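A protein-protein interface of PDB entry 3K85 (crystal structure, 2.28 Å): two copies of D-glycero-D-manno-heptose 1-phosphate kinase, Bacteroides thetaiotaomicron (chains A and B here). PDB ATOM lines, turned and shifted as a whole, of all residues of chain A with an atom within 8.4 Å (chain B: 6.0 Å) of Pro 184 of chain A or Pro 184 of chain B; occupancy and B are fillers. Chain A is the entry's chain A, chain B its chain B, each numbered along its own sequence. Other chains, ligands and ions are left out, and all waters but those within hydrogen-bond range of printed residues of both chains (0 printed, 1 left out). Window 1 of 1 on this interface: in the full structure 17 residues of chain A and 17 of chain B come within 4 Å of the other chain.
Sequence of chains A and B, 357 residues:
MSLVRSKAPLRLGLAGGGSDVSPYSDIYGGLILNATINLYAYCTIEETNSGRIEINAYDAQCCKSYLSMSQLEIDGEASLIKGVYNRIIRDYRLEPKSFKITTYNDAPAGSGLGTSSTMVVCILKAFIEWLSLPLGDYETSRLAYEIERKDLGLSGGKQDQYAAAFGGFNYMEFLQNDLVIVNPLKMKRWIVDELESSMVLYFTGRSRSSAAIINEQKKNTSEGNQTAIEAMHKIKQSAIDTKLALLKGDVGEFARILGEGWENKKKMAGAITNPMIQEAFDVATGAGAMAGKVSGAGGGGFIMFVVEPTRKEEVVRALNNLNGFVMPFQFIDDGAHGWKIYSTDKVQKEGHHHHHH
The backbone carbonyl oxygen (O) of Pro 184 of chain A is in hydrogen-bond range of the backbone NH (N) of Lys 186 of chain B, 2.8 Å away.
The backbone NH (N) of Lys 186 of chain A sits at hydrogen-bond distance from the backbone carbonyl oxygen (O) of Pro 184 of chain B (2.7 Å).
The side-chain amino group (NZ) of Lys 243 of chain A sits at hydrogen-bond distance from the side-chain amide oxygen (OD1) of Asn 183 of chain B.
The side-chain amino group (NZ) of Lys 186 of chain B is in salt-bridge range of the side-chain carboxylate (OD2) of Asp 333 of chain A, at 2.9 Å.
Gly 167 of chain A touches Lys 186 of chain B, and with the chains exchanged Lys 186 of chain A touches Gly 167 of chain B.
Pro 184 of chain A touches Leu 185 of chain B, and with the chains exchanged Leu 185 of chain A touches Pro 184 of chain B.
Pro 184 of chain A touches Leu 247 of chain B, but with the chains exchanged Leu 247 of chain A does not touch Pro 184 of chain B (4.1 Å).
Lys 186 of chain B touches its own counterpart, Lys 186 of chain A.
Of the 17 pairs that touch across the chains among the printed residues, 14 have their exchanged pair printed and touching as well.
Hydrophobic or aromatic side chains of chain B that line the printed part of chain A: Pro 184 and Leu 247.
Hydrophobic or aromatic side chains of chain A within 4 Å of the printed part of chain B: Pro 184, Leu 185 and Leu 247.
Among the printed residues, 17 pairs touch across the chains.
Among the printed residues, Asp or Glu carboxylates within 4 Å of a Lys or Arg side-chain nitrogen of the other chain: Asp 333 of chain A with Lys 186 of chain B (2.9 Å).
Among the printed residues, merely in contact across the chains: Gly 167 of chain A with Lys 186 of chain B (3.9 Å), Val 182 of chain A with Leu 247 of chain B (3.2 Å), Asn 183 of chain A with Leu 247 of chain B (3.8 Å), Pro 184 of chain A with Pro 184 of chain B (3.5 Å), Pro 184 of chain A with Leu 185 of chain B (3.3 Å), Pro 184 of chain A with Leu 247 of chain B (3.6 Å), Leu 185 of chain A with Pro 184 of chain B (3.2 Å), Leu 185 of chain A with Lys 186 of chain B (3.9 Å), Lys 186 of chain A with Gly 167 of chain B (3.6 Å), Lys 186 of chain A with Leu 185 of chain B (3.6 Å), Lys 186 of chain A with Lys 186 of chain B (3.3 Å), Leu 247 of chain A with Val 182 of chain B (3.6 Å) and Leu 247 of chain A with Asn 183 of chain B (3.8 Å).
Of chain B, only Pro 184, Leu 185, Lys 186 and Leu 247 come within 4 Å of Pro 184 of chain A.
Of chain A, only Pro 184, Leu 185 and Lys 186 come within 4 Å of Pro 184 of chain B.
Printed residues of chain B within 4 Å of Lys 186 of chain A: Gly 167 (3.6 Å), Pro 184 (2.7 Å), Leu 185 (3.6 Å) and Lys 186 (3.3 Å).
Of the printed residues of chain B, Asp 333 of chain A touches Lys 186 (2.9 Å).
Printed residues of chain A within 4 Å of Leu 185 of chain B: Pro 184 (3.3 Å) and Lys 186 (3.6 Å).
Asn 170 of chain A touches none of the printed residues of chain B.
The nearest residue of chain B that does not touch Pro 184 of chain A is Met 187 of chain B (5.7 Å).
The nearest printed residue of chain A that does not touch Val 182 of chain B is Lys 248 of chain A (5.8 Å).
The backbone NH (N) of Val 182 of chain A sits at hydrogen-bond distance from the side-chain hydroxyl (OH) of Tyr 138 of chain A.
The backbone carbonyl oxygen (O) of Gly 167 of chain A sits close to the side-chain amide oxygen (OD1) of Asn 170 of chain A.
The backbone NH (N) of Gly 168 of chain A lies within hydrogen-bond range of the backbone carbonyl oxygen (O) of Asp 333 of chain A.
The backbone NH (N) of Leu 185 of chain A sits at hydrogen-bond distance from the backbone carbonyl oxygen (O) of Phe 169 of chain A (2.9 Å).
The side-chain amide oxygen (OD1) of Asn 170 of chain B sits close to the backbone carbonyl oxygen (O) of Gly 167 of chain B (2.9 Å).
O of Phe 169 of chain B lies within hydrogen-bond range of N of Leu 185 of chain B (2.9 Å).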
ATOM      1  N   ASP A 137      11.344 -10.706  23.301  1.00  0.00           N
ATOM      2  CA  ASP A 137      12.234 -10.050  24.248  1.00  0.00           C
ATOM      3  C   ASP A 137      11.533  -9.597  25.517  1.00  0.00           C
ATOM      4  O   ASP A 137      11.825 -10.105  26.600  1.00  0.00           O
ATOM      5  CB  ASP A 137      12.924  -8.847  23.611  1.00  0.00           C
ATOM      6  CG  ASP A 137      13.815  -9.230  22.457  1.00  0.00           C
ATOM      7  OD1 ASP A 137      14.421 -10.322  22.500  1.00  0.00           O
ATOM      8  OD2 ASP A 137      13.919  -8.424  21.507  1.00  0.00           O
ATOM      9  N   TYR A 138      10.618  -8.640  25.398  1.00  0.00           N
ATOM     10  CA  TYR A 138       9.925  -8.143  26.578  1.00  0.00           C
ATOM     11  C   TYR A 138       9.313  -9.234  27.442  1.00  0.00           C
ATOM     12  O   TYR A 138       9.517  -9.243  28.644  1.00  0.00           O
ATOM     13  CB  TYR A 138       8.872  -7.099  26.185  1.00  0.00           C
ATOM     14  CG  TYR A 138       9.474  -5.720  25.996  1.00  0.00           C
ATOM     15  CD1 TYR A 138       9.825  -4.939  27.097  1.00  0.00           C
ATOM     16  CD2 TYR A 138       9.728  -5.213  24.715  1.00  0.00           C
ATOM     17  CE1 TYR A 138      10.419  -3.668  26.931  1.00  0.00           C
ATOM     18  CE2 TYR A 138      10.318  -3.946  24.533  1.00  0.00           C
ATOM     19  CZ  TYR A 138      10.657  -3.179  25.642  1.00  0.00           C
ATOM     20  OH  TYR A 138      11.193  -1.920  25.465  1.00  0.00           O
ATOM     21  N   PHE A 166      17.894  -8.900  25.640  1.00  0.00           N
ATOM     22  CA  PHE A 166      18.007  -7.887  24.591  1.00  0.00           C
ATOM     23  C   PHE A 166      19.363  -7.801  23.901  1.00  0.00           C
ATOM     24  O   PHE A 166      19.411  -7.758  22.674  1.00  0.00           O
ATOM     25  CB  PHE A 166      17.598  -6.520  25.147  1.00  0.00           C
ATOM     26  CG  PHE A 166      16.109  -6.365  25.304  1.00  0.00           C
ATOM     27  CD1 PHE A 166      15.348  -5.727  24.318  1.00  0.00           C
ATOM     28  CD2 PHE A 166      15.455  -6.891  26.423  1.00  0.00           C
ATOM     29  CE1 PHE A 166      13.958  -5.611  24.447  1.00  0.00           C
ATOM     30  CE2 PHE A 166      14.070  -6.781  26.563  1.00  0.00           C
ATOM     31  CZ  PHE A 166      13.316  -6.138  25.571  1.00  0.00           C
ATOM     32  N   GLY A 167      20.451  -7.772  24.675  1.00  0.00           N
ATOM     33  CA  GLY A 167      21.785  -7.704  24.095  1.00  0.00           C
ATOM     34  C   GLY A 167      22.207  -6.320  23.640  1.00  0.00           C
ATOM     35  O   GLY A 167      21.355  -5.452  23.402  1.00  0.00           O
ATOM     36  N   GLY A 168      23.523  -6.117  23.528  1.00  0.00           N
ATOM     37  CA  GLY A 168      24.088  -4.841  23.094  1.00  0.00           C
ATOM     38  C   GLY A 168      24.181  -3.766  24.171  1.00  0.00           C
ATOM     39  O   GLY A 168      24.204  -4.080  25.359  1.00  0.00           O
ATOM     40  N   PHE A 169      24.284  -2.500  23.751  1.00  0.00           N
ATOM     41  CA  PHE A 169      24.311  -1.359  24.673  1.00  0.00           C
ATOM     42  C   PHE A 169      22.851  -0.874  24.803  1.00  0.00           C
ATOM     43  O   PHE A 169      22.240  -0.417  23.829  1.00  0.00           O
ATOM     44  CB  PHE A 169      25.170  -0.214  24.123  1.00  0.00           C
ATOM     45  CG  PHE A 169      26.645  -0.433  24.266  1.00  0.00           C
ATOM     46  CD1 PHE A 169      27.385   0.305  25.185  1.00  0.00           C
ATOM     47  CD2 PHE A 169      27.298  -1.396  23.499  1.00  0.00           C
ATOM     48  CE1 PHE A 169      28.754   0.081  25.340  1.00  0.00           C
ATOM     49  CE2 PHE A 169      28.668  -1.627  23.649  1.00  0.00           C
ATOM     50  CZ  PHE A 169      29.393  -0.890  24.569  1.00  0.00           C
ATOM     51  N   ASN A 170      22.295  -0.989  26.003  1.00  0.00           N
ATOM     52  CA  ASN A 170      20.915  -0.590  26.248  1.00  0.00           C
ATOM     53  C   ASN A 170      20.804   0.519  27.308  1.00  0.00           C
ATOM     54  O   ASN A 170      21.629   0.618  28.217  1.00  0.00           O
ATOM     55  CB  ASN A 170      20.092  -1.817  26.682  1.00  0.00           C
ATOM     56  CG  ASN A 170      19.885  -2.817  25.548  1.00  0.00           C
ATOM     57  OD1 ASN A 170      20.136  -4.018  25.697  1.00  0.00           O
ATOM     58  ND2 ASN A 170      19.410  -2.324  24.405  1.00  0.00           N
ATOM     59  N   TYR A 171      19.802   1.375  27.142  1.00  0.00           N
ATOM     60  CA  TYR A 171      19.508   2.450  28.088  1.00  0.00           C
ATOM     61  C   TYR A 171      18.089   2.070  28.463  1.00  0.00           C
ATOM     62  O   TYR A 171      17.163   2.222  27.667  1.00  0.00           O
ATOM     63  CB  TYR A 171      19.528   3.803  27.398  1.00  0.00           C
ATOM     64  CG  TYR A 171      19.238   4.988  28.296  1.00  0.00           C
ATOM     65  CD1 TYR A 171      20.214   5.495  29.147  1.00  0.00           C
ATOM     66  CD2 TYR A 171      18.006   5.649  28.240  1.00  0.00           C
ATOM     67  CE1 TYR A 171      19.985   6.636  29.915  1.00  0.00           C
ATOM     68  CE2 TYR A 171      17.766   6.786  29.002  1.00  0.00           C
ATOM     69  CZ  TYR A 171      18.764   7.272  29.838  1.00  0.00           C
ATOM     70  OH  TYR A 171      18.546   8.388  30.606  1.00  0.00           O
ATOM     71  N   MET A 172      17.934   1.538  29.665  1.00  0.00           N
ATOM     72  CA  MET A 172      16.643   1.067  30.137  1.00  0.00           C
ATOM     73  C   MET A 172      15.962   2.020  31.096  1.00  0.00           C
ATOM     74  O   MET A 172      16.596   2.608  31.980  1.00  0.00           O
ATOM     75  CB  MET A 172      16.812  -0.292  30.817  1.00  0.00           C
ATOM     76  CG  MET A 172      17.802  -1.197  30.102  1.00  0.00           C
ATOM     77  SD  MET A 172      17.953  -2.972  30.852  1.00  0.00           S
ATOM     78  CE  MET A 172      18.051  -3.982  29.176  1.00  0.00           C
ATOM     79  N   ILE A 181      11.043   0.258  29.597  1.00  0.00           N
ATOM     80  CA  ILE A 181      11.328   0.613  28.217  1.00  0.00           C
ATOM     81  C   ILE A 181      12.798   0.370  27.938  1.00  0.00           C
ATOM     82  O   ILE A 181      13.665   0.864  28.654  1.00  0.00           O
ATOM     83  CB  ILE A 181      11.036   2.107  27.922  1.00  0.00           C
ATOM     84  CG1 ILE A 181       9.639   2.482  28.424  1.00  0.00           C
ATOM     85  CG2 ILE A 181      11.143   2.369  26.431  1.00  0.00           C
ATOM     86  CD1 ILE A 181       8.543   1.544  27.949  1.00  0.00           C
ATOM     87  N   VAL A 182      13.081  -0.402  26.903  1.00  0.00           N
ATOM     88  CA  VAL A 182      14.465  -0.666  26.532  1.00  0.00           C
ATOM     89  C   VAL A 182      14.796   0.094  25.245  1.00  0.00           C
ATOM     90  O   VAL A 182      14.189  -0.144  24.202  1.00  0.00           O
ATOM     91  CB  VAL A 182      14.709  -2.171  26.305  1.00  0.00           C
ATOM     92  CG1 VAL A 182      16.157  -2.414  25.904  1.00  0.00           C
ATOM     93  CG2 VAL A 182      14.368  -2.938  27.566  1.00  0.00           C
ATOM     94  N   ASN A 183      15.722   1.040  25.341  1.00  0.00           N
ATOM     95  CA  ASN A 183      16.155   1.802  24.176  1.00  0.00           C
ATOM     96  C   ASN A 183      17.415   1.103  23.662  1.00  0.00           C
ATOM     97  O   ASN A 183      18.511   1.336  24.172  1.00  0.00           O
ATOM     98  CB  ASN A 183      16.478   3.248  24.576  1.00  0.00           C
ATOM     99  CG  ASN A 183      15.257   4.004  25.056  1.00  0.00           C
ATOM    100  OD1 ASN A 183      14.460   4.487  24.259  1.00  0.00           O
ATOM    101  ND2 ASN A 183      15.094   4.095  26.375  1.00  0.00           N
ATOM    102  N   PRO A 184      17.269   0.211  22.666  1.00  0.00           N
ATOM    103  CA  PRO A 184      18.424  -0.510  22.108  1.00  0.00           C
ATOM    104  C   PRO A 184      19.292   0.485  21.362  1.00  0.00           C
ATOM    105  O   PRO A 184      18.878   1.000  20.330  1.00  0.00           O
ATOM    106  CB  PRO A 184      17.785  -1.517  21.145  1.00  0.00           C
ATOM    107  CG  PRO A 184      16.350  -1.629  21.617  1.00  0.00           C
ATOM    108  CD  PRO A 184      16.020  -0.213  22.009  1.00  0.00           C
ATOM    109  N   LEU A 185      20.491   0.758  21.863  1.00  0.00           N
ATOM    110  CA  LEU A 185      21.364   1.731  21.207  1.00  0.00           C
ATOM    111  C   LEU A 185      22.361   1.173  20.186  1.00  0.00           C
ATOM    112  O   LEU A 185      23.117   0.256  20.499  1.00  0.00           O
ATOM    113  CB  LEU A 185      22.161   2.514  22.259  1.00  0.00           C
ATOM    114  CG  LEU A 185      21.446   3.253  23.393  1.00  0.00           C
ATOM    115  CD1 LEU A 185      22.506   3.866  24.315  1.00  0.00           C
ATOM    116  CD2 LEU A 185      20.538   4.337  22.833  1.00  0.00           C
ATOM    117  N   LYS A 186      22.365   1.727  18.973  1.00  0.00           N
ATOM    118  CA  LYS A 186      23.339   1.311  17.964  1.00  0.00           C
ATOM    119  C   LYS A 186      24.641   1.983  18.377  1.00  0.00           C
ATOM    120  O   LYS A 186      24.689   3.199  18.505  1.00  0.00           O
ATOM    121  CB  LYS A 186      22.988   1.826  16.561  1.00  0.00           C
ATOM    122  CG  LYS A 186      21.831   1.151  15.868  1.00  0.00           C
ATOM    123  CD  LYS A 186      21.904   1.335  14.347  1.00  0.00           C
ATOM    124  CE  LYS A 186      22.057   2.796  13.949  1.00  0.00           C
ATOM    125  NZ  LYS A 186      21.847   2.991  12.497  1.00  0.00           N
ATOM    126  N   MET A 187      25.697   1.219  18.598  1.00  0.00           N
ATOM    127  CA  MET A 187      26.953   1.844  18.978  1.00  0.00           C
ATOM    128  C   MET A 187      27.946   1.800  17.826  1.00  0.00           C
ATOM    129  O   MET A 187      28.230   0.730  17.293  1.00  0.00           O
ATOM    130  CB  MET A 187      27.546   1.153  20.209  1.00  0.00           C
ATOM    131  CG  MET A 187      26.824   1.466  21.512  1.00  0.00           C
ATOM    132  SD  MET A 187      26.986   3.332  22.120  1.00  0.00           S
ATOM    133  CE  MET A 187      28.856   3.316  22.590  1.00  0.00           C
ATOM    134  N   LYS A 188      28.452   2.960  17.423  1.00  0.00           N
ATOM    135  CA  LYS A 188      29.444   3.001  16.354  1.00  0.00           C
ATOM    136  C   LYS A 188      30.616   2.073  16.720  1.00  0.00           C
ATOM    137  O   LYS A 188      31.072   2.056  17.858  1.00  0.00           O
ATOM    138  CB  LYS A 188      29.932   4.439  16.135  1.00  0.00           C
ATOM    139  CG  LYS A 188      28.853   5.346  15.541  1.00  0.00           C
ATOM    140  CD  LYS A 188      29.439   6.483  14.715  1.00  0.00           C
ATOM    141  CE  LYS A 188      30.139   7.533  15.586  1.00  0.00           C
ATOM    142  NZ  LYS A 188      29.187   8.349  16.406  1.00  0.00           N
ATOM    143  N   ILE A 191      33.647   3.420  18.701  1.00  0.00           N
ATOM    144  CA  ILE A 191      33.425   3.778  20.108  1.00  0.00           C
ATOM    145  C   ILE A 191      33.564   2.505  20.944  1.00  0.00           C
ATOM    146  O   ILE A 191      34.163   2.502  22.024  1.00  0.00           O
ATOM    147  CB  ILE A 191      32.010   4.391  20.315  1.00  0.00           C
ATOM    148  CG1 ILE A 191      31.945   5.759  19.632  1.00  0.00           C
ATOM    149  CG2 ILE A 191      31.684   4.505  21.800  1.00  0.00           C
ATOM    150  CD1 ILE A 191      30.566   6.363  19.647  1.00  0.00           C
ATOM    151  N   LYS A 243      25.294   7.870  29.231  1.00  0.00           N
ATOM    152  CA  LYS A 243      24.754   7.606  27.902  1.00  0.00           C
ATOM    153  C   LYS A 243      25.283   8.662  26.946  1.00  0.00           C
ATOM    154  O   LYS A 243      25.905   8.352  25.925  1.00  0.00           O
ATOM    155  CB  LYS A 243      23.226   7.667  27.901  1.00  0.00           C
ATOM    156  CG  LYS A 243      22.624   7.355  26.538  1.00  0.00           C
ATOM    157  CD  LYS A 243      21.124   7.554  26.512  1.00  0.00           C
ATOM    158  CE  LYS A 243      20.757   9.018  26.667  1.00  0.00           C
ATOM    159  NZ  LYS A 243      19.304   9.228  26.432  1.00  0.00           N
ATOM    160  N   LEU A 247      27.938   7.964  23.776  1.00  0.00           N
ATOM    161  CA  LEU A 247      27.383   8.085  22.435  1.00  0.00           C
ATOM    162  C   LEU A 247      28.286   8.958  21.567  1.00  0.00           C
ATOM    163  O   LEU A 247      28.216   8.911  20.337  1.00  0.00           O
ATOM    164  CB  LEU A 247      25.982   8.695  22.480  1.00  0.00           C
ATOM    165  CG  LEU A 247      24.848   7.802  22.979  1.00  0.00           C
ATOM    166  CD1 LEU A 247      23.537   8.574  22.915  1.00  0.00           C
ATOM    167  CD2 LEU A 247      24.777   6.538  22.134  1.00  0.00           C
ATOM    168  N   LYS A 248      29.124   9.764  22.214  1.00  0.00           N
ATOM    169  CA  LYS A 248      30.044  10.647  21.506  1.00  0.00           C
ATOM    170  C   LYS A 248      31.471  10.083  21.516  1.00  0.00           C
ATOM    171  O   LYS A 248      32.362  10.620  20.860  1.00  0.00           O
ATOM    172  CB  LYS A 248      30.025  12.052  22.132  1.00  0.00           C
ATOM    173  CG  LYS A 248      28.767  12.865  21.812  1.00  0.00           C
ATOM    174  CD  LYS A 248      28.900  14.317  22.283  1.00  0.00           C
ATOM    175  CE  LYS A 248      27.897  15.261  21.593  1.00  0.00           C
ATOM    176  NZ  LYS A 248      26.468  15.009  21.960  1.00  0.00           N
ATOM    177  N   ASP A 333      27.019  -7.494  20.754  1.00  0.00           N
ATOM    178  CA  ASP A 333      25.777  -6.782  20.452  1.00  0.00           C
ATOM    179  C   ASP A 333      24.496  -7.598  20.433  1.00  0.00           C
ATOM    180  O   ASP A 333      23.405  -7.030  20.418  1.00  0.00           O
ATOM    181  CB  ASP A 333      25.886  -6.050  19.113  1.00  0.00           C
ATOM    182  CG  ASP A 333      24.695  -5.131  18.861  1.00  0.00           C
ATOM    183  OD1 ASP A 333      24.592  -4.091  19.547  1.00  0.00           O
ATOM    184  OD2 ASP A 333      23.854  -5.453  17.988  1.00  0.00           O
ATOM    185  N   PHE B 166      23.487  10.694  10.306  1.00  0.00           N
ATOM    186  CA  PHE B 166      23.501   9.543  11.197  1.00  0.00           C
ATOM    187  C   PHE B 166      22.899   8.267  10.638  1.00  0.00           C
ATOM    188  O   PHE B 166      23.487   7.200  10.801  1.00  0.00           O
ATOM    189  CB  PHE B 166      22.817   9.913  12.519  1.00  0.00           C
ATOM    190  CG  PHE B 166      23.671  10.783  13.420  1.00  0.00           C
ATOM    191  CD1 PHE B 166      24.374  10.225  14.492  1.00  0.00           C
ATOM    192  CD2 PHE B 166      23.784  12.151  13.188  1.00  0.00           C
ATOM    193  CE1 PHE B 166      25.176  11.019  15.321  1.00  0.00           C
ATOM    194  CE2 PHE B 166      24.582  12.955  14.010  1.00  0.00           C
ATOM    195  CZ  PHE B 166      25.280  12.383  15.081  1.00  0.00           C
ATOM    196  N   GLY B 167      21.726   8.365  10.007  1.00  0.00           N
ATOM    197  CA  GLY B 167      21.082   7.190   9.424  1.00  0.00           C
ATOM    198  C   GLY B 167      20.326   6.276  10.380  1.00  0.00           C
ATOM    199  O   GLY B 167      20.572   6.275  11.584  1.00  0.00           O
ATOM    200  N   PHE B 169      16.983   4.538  12.417  1.00  0.00           N
ATOM    201  CA  PHE B 169      15.915   5.034  13.285  1.00  0.00           C
ATOM    202  C   PHE B 169      16.609   5.803  14.409  1.00  0.00           C
ATOM    203  O   PHE B 169      17.427   5.235  15.147  1.00  0.00           O
ATOM    204  CB  PHE B 169      15.115   3.877  13.890  1.00  0.00           C
ATOM    205  CG  PHE B 169      14.076   3.311  12.979  1.00  0.00           C
ATOM    206  CD1 PHE B 169      12.727   3.604  13.181  1.00  0.00           C
ATOM    207  CD2 PHE B 169      14.442   2.504  11.904  1.00  0.00           C
ATOM    208  CE1 PHE B 169      11.748   3.101  12.322  1.00  0.00           C
ATOM    209  CE2 PHE B 169      13.481   1.994  11.035  1.00  0.00           C
ATOM    210  CZ  PHE B 169      12.130   2.291  11.240  1.00  0.00           C
ATOM    211  N   ASN B 170      16.271   7.085  14.541  1.00  0.00           N
ATOM    212  CA  ASN B 170      16.876   7.948  15.545  1.00  0.00           C
ATOM    213  C   ASN B 170      15.878   8.695  16.423  1.00  0.00           C
ATOM    214  O   ASN B 170      14.812   9.108  15.971  1.00  0.00           O
ATOM    215  CB  ASN B 170      17.791   8.962  14.854  1.00  0.00           C
ATOM    216  CG  ASN B 170      19.031   8.323  14.264  1.00  0.00           C
ATOM    217  OD1 ASN B 170      19.333   8.484  13.075  1.00  0.00           O
ATOM    218  ND2 ASN B 170      19.771   7.601  15.099  1.00  0.00           N
ATOM    219  N   TYR B 171      16.236   8.850  17.692  1.00  0.00           N
ATOM    220  CA  TYR B 171      15.412   9.586  18.639  1.00  0.00           C
ATOM    221  C   TYR B 171      16.283  10.792  18.966  1.00  0.00           C
ATOM    222  O   TYR B 171      17.326  10.660  19.615  1.00  0.00           O
ATOM    223  CB  TYR B 171      15.152   8.762  19.890  1.00  0.00           C
ATOM    224  CG  TYR B 171      14.226   9.447  20.859  1.00  0.00           C
ATOM    225  CD1 TYR B 171      12.905   9.733  20.502  1.00  0.00           C
ATOM    226  CD2 TYR B 171      14.654   9.795  22.141  1.00  0.00           C
ATOM    227  CE1 TYR B 171      12.031  10.341  21.398  1.00  0.00           C
ATOM    228  CE2 TYR B 171      13.787  10.403  23.040  1.00  0.00           C
ATOM    229  CZ  TYR B 171      12.472  10.671  22.659  1.00  0.00           C
ATOM    230  OH  TYR B 171      11.598  11.264  23.543  1.00  0.00           O
ATOM    231  N   VAL B 182      21.644  12.634  19.684  1.00  0.00           N
ATOM    232  CA  VAL B 182      21.071  11.643  18.775  1.00  0.00           C
ATOM    233  C   VAL B 182      21.152  10.282  19.458  1.00  0.00           C
ATOM    234  O   VAL B 182      22.238   9.786  19.755  1.00  0.00           O
ATOM    235  CB  VAL B 182      21.837  11.568  17.414  1.00  0.00           C
ATOM    236  CG1 VAL B 182      21.222  10.495  16.518  1.00  0.00           C
ATOM    237  CG2 VAL B 182      21.770  12.906  16.700  1.00  0.00           C
ATOM    238  N   ASN B 183      19.997   9.693  19.735  1.00  0.00           N
ATOM    239  CA  ASN B 183      19.946   8.371  20.347  1.00  0.00           C
ATOM    240  C   ASN B 183      19.699   7.368  19.217  1.00  0.00           C
ATOM    241  O   ASN B 183      18.559   7.169  18.798  1.00  0.00           O
ATOM    242  CB  ASN B 183      18.800   8.306  21.358  1.00  0.00           C
ATOM    243  CG  ASN B 183      19.001   9.248  22.528  1.00  0.00           C
ATOM    244  OD1 ASN B 183      19.758   8.961  23.445  1.00  0.00           O
ATOM    245  ND2 ASN B 183      18.326  10.387  22.495  1.00  0.00           N
ATOM    246  N   PRO B 184      20.770   6.743  18.695  1.00  0.00           N
ATOM    247  CA  PRO B 184      20.708   5.754  17.607  1.00  0.00           C
ATOM    248  C   PRO B 184      19.999   4.484  18.053  1.00  0.00           C
ATOM    249  O   PRO B 184      20.546   3.698  18.824  1.00  0.00           O
ATOM    250  CB  PRO B 184      22.184   5.485  17.285  1.00  0.00           C
ATOM    251  CG  PRO B 184      22.883   6.723  17.758  1.00  0.00           C
ATOM    252  CD  PRO B 184      22.171   7.020  19.056  1.00  0.00           C
ATOM    253  N   LEU B 185      18.789   4.276  17.563  1.00  0.00           N
ATOM    254  CA  LEU B 185      18.028   3.099  17.938  1.00  0.00           C
ATOM    255  C   LEU B 185      18.263   1.903  17.021  1.00  0.00           C
ATOM    256  O   LEU B 185      18.325   2.044  15.799  1.00  0.00           O
ATOM    257  CB  LEU B 185      16.526   3.413  17.945  1.00  0.00           C
ATOM    258  CG  LEU B 185      16.020   4.552  18.825  1.00  0.00           C
ATOM    259  CD1 LEU B 185      14.495   4.628  18.732  1.00  0.00           C
ATOM    260  CD2 LEU B 185      16.450   4.315  20.257  1.00  0.00           C
ATOM    261  N   LYS B 186      18.413   0.727  17.620  1.00  0.00           N
ATOM    262  CA  LYS B 186      18.551  -0.492  16.843  1.00  0.00           C
ATOM    263  C   LYS B 186      17.112  -0.936  16.698  1.00  0.00           C
ATOM    264  O   LYS B 186      16.337  -0.858  17.649  1.00  0.00           O
ATOM    265  CB  LYS B 186      19.305  -1.577  17.598  1.00  0.00           C
ATOM    266  CG  LYS B 186      20.793  -1.365  17.736  1.00  0.00           C
ATOM    267  CD  LYS B 186      21.483  -2.695  18.028  1.00  0.00           C
ATOM    268  CE  LYS B 186      20.823  -3.413  19.200  1.00  0.00           C
ATOM    269  NZ  LYS B 186      21.548  -4.652  19.540  1.00  0.00           N
ATOM    270  N   MET B 187      16.735  -1.389  15.520  1.00  0.00           N
ATOM    271  CA  MET B 187      15.370  -1.833  15.334  1.00  0.00           C
ATOM    272  C   MET B 187      15.347  -3.299  14.945  1.00  0.00           C
ATOM    273  O   MET B 187      15.948  -3.678  13.942  1.00  0.00           O
ATOM    274  CB  MET B 187      14.698  -0.991  14.256  1.00  0.00           C
ATOM    275  CG  MET B 187      14.324   0.423  14.715  1.00  0.00           C
ATOM    276  SD  MET B 187      12.957   0.512  16.141  1.00  0.00           S
ATOM    277  CE  MET B 187      11.394  -0.004  15.141  1.00  0.00           C
ATOM    278  N   LEU B 247       9.148   0.581  19.449  1.00  0.00           N
ATOM    279  CA  LEU B 247      10.170  -0.273  20.054  1.00  0.00           C
ATOM    280  C   LEU B 247       9.551  -1.613  20.421  1.00  0.00           C
ATOM    281  O   LEU B 247      10.225  -2.644  20.434  1.00  0.00           O
ATOM    282  CB  LEU B 247      10.752   0.371  21.315  1.00  0.00           C
ATOM    283  CG  LEU B 247      11.868   1.387  21.086  1.00  0.00           C
ATOM    284  CD1 LEU B 247      12.383   1.871  22.426  1.00  0.00           C
ATOM    285  CD2 LEU B 247      13.000   0.743  20.284  1.00  0.00           C
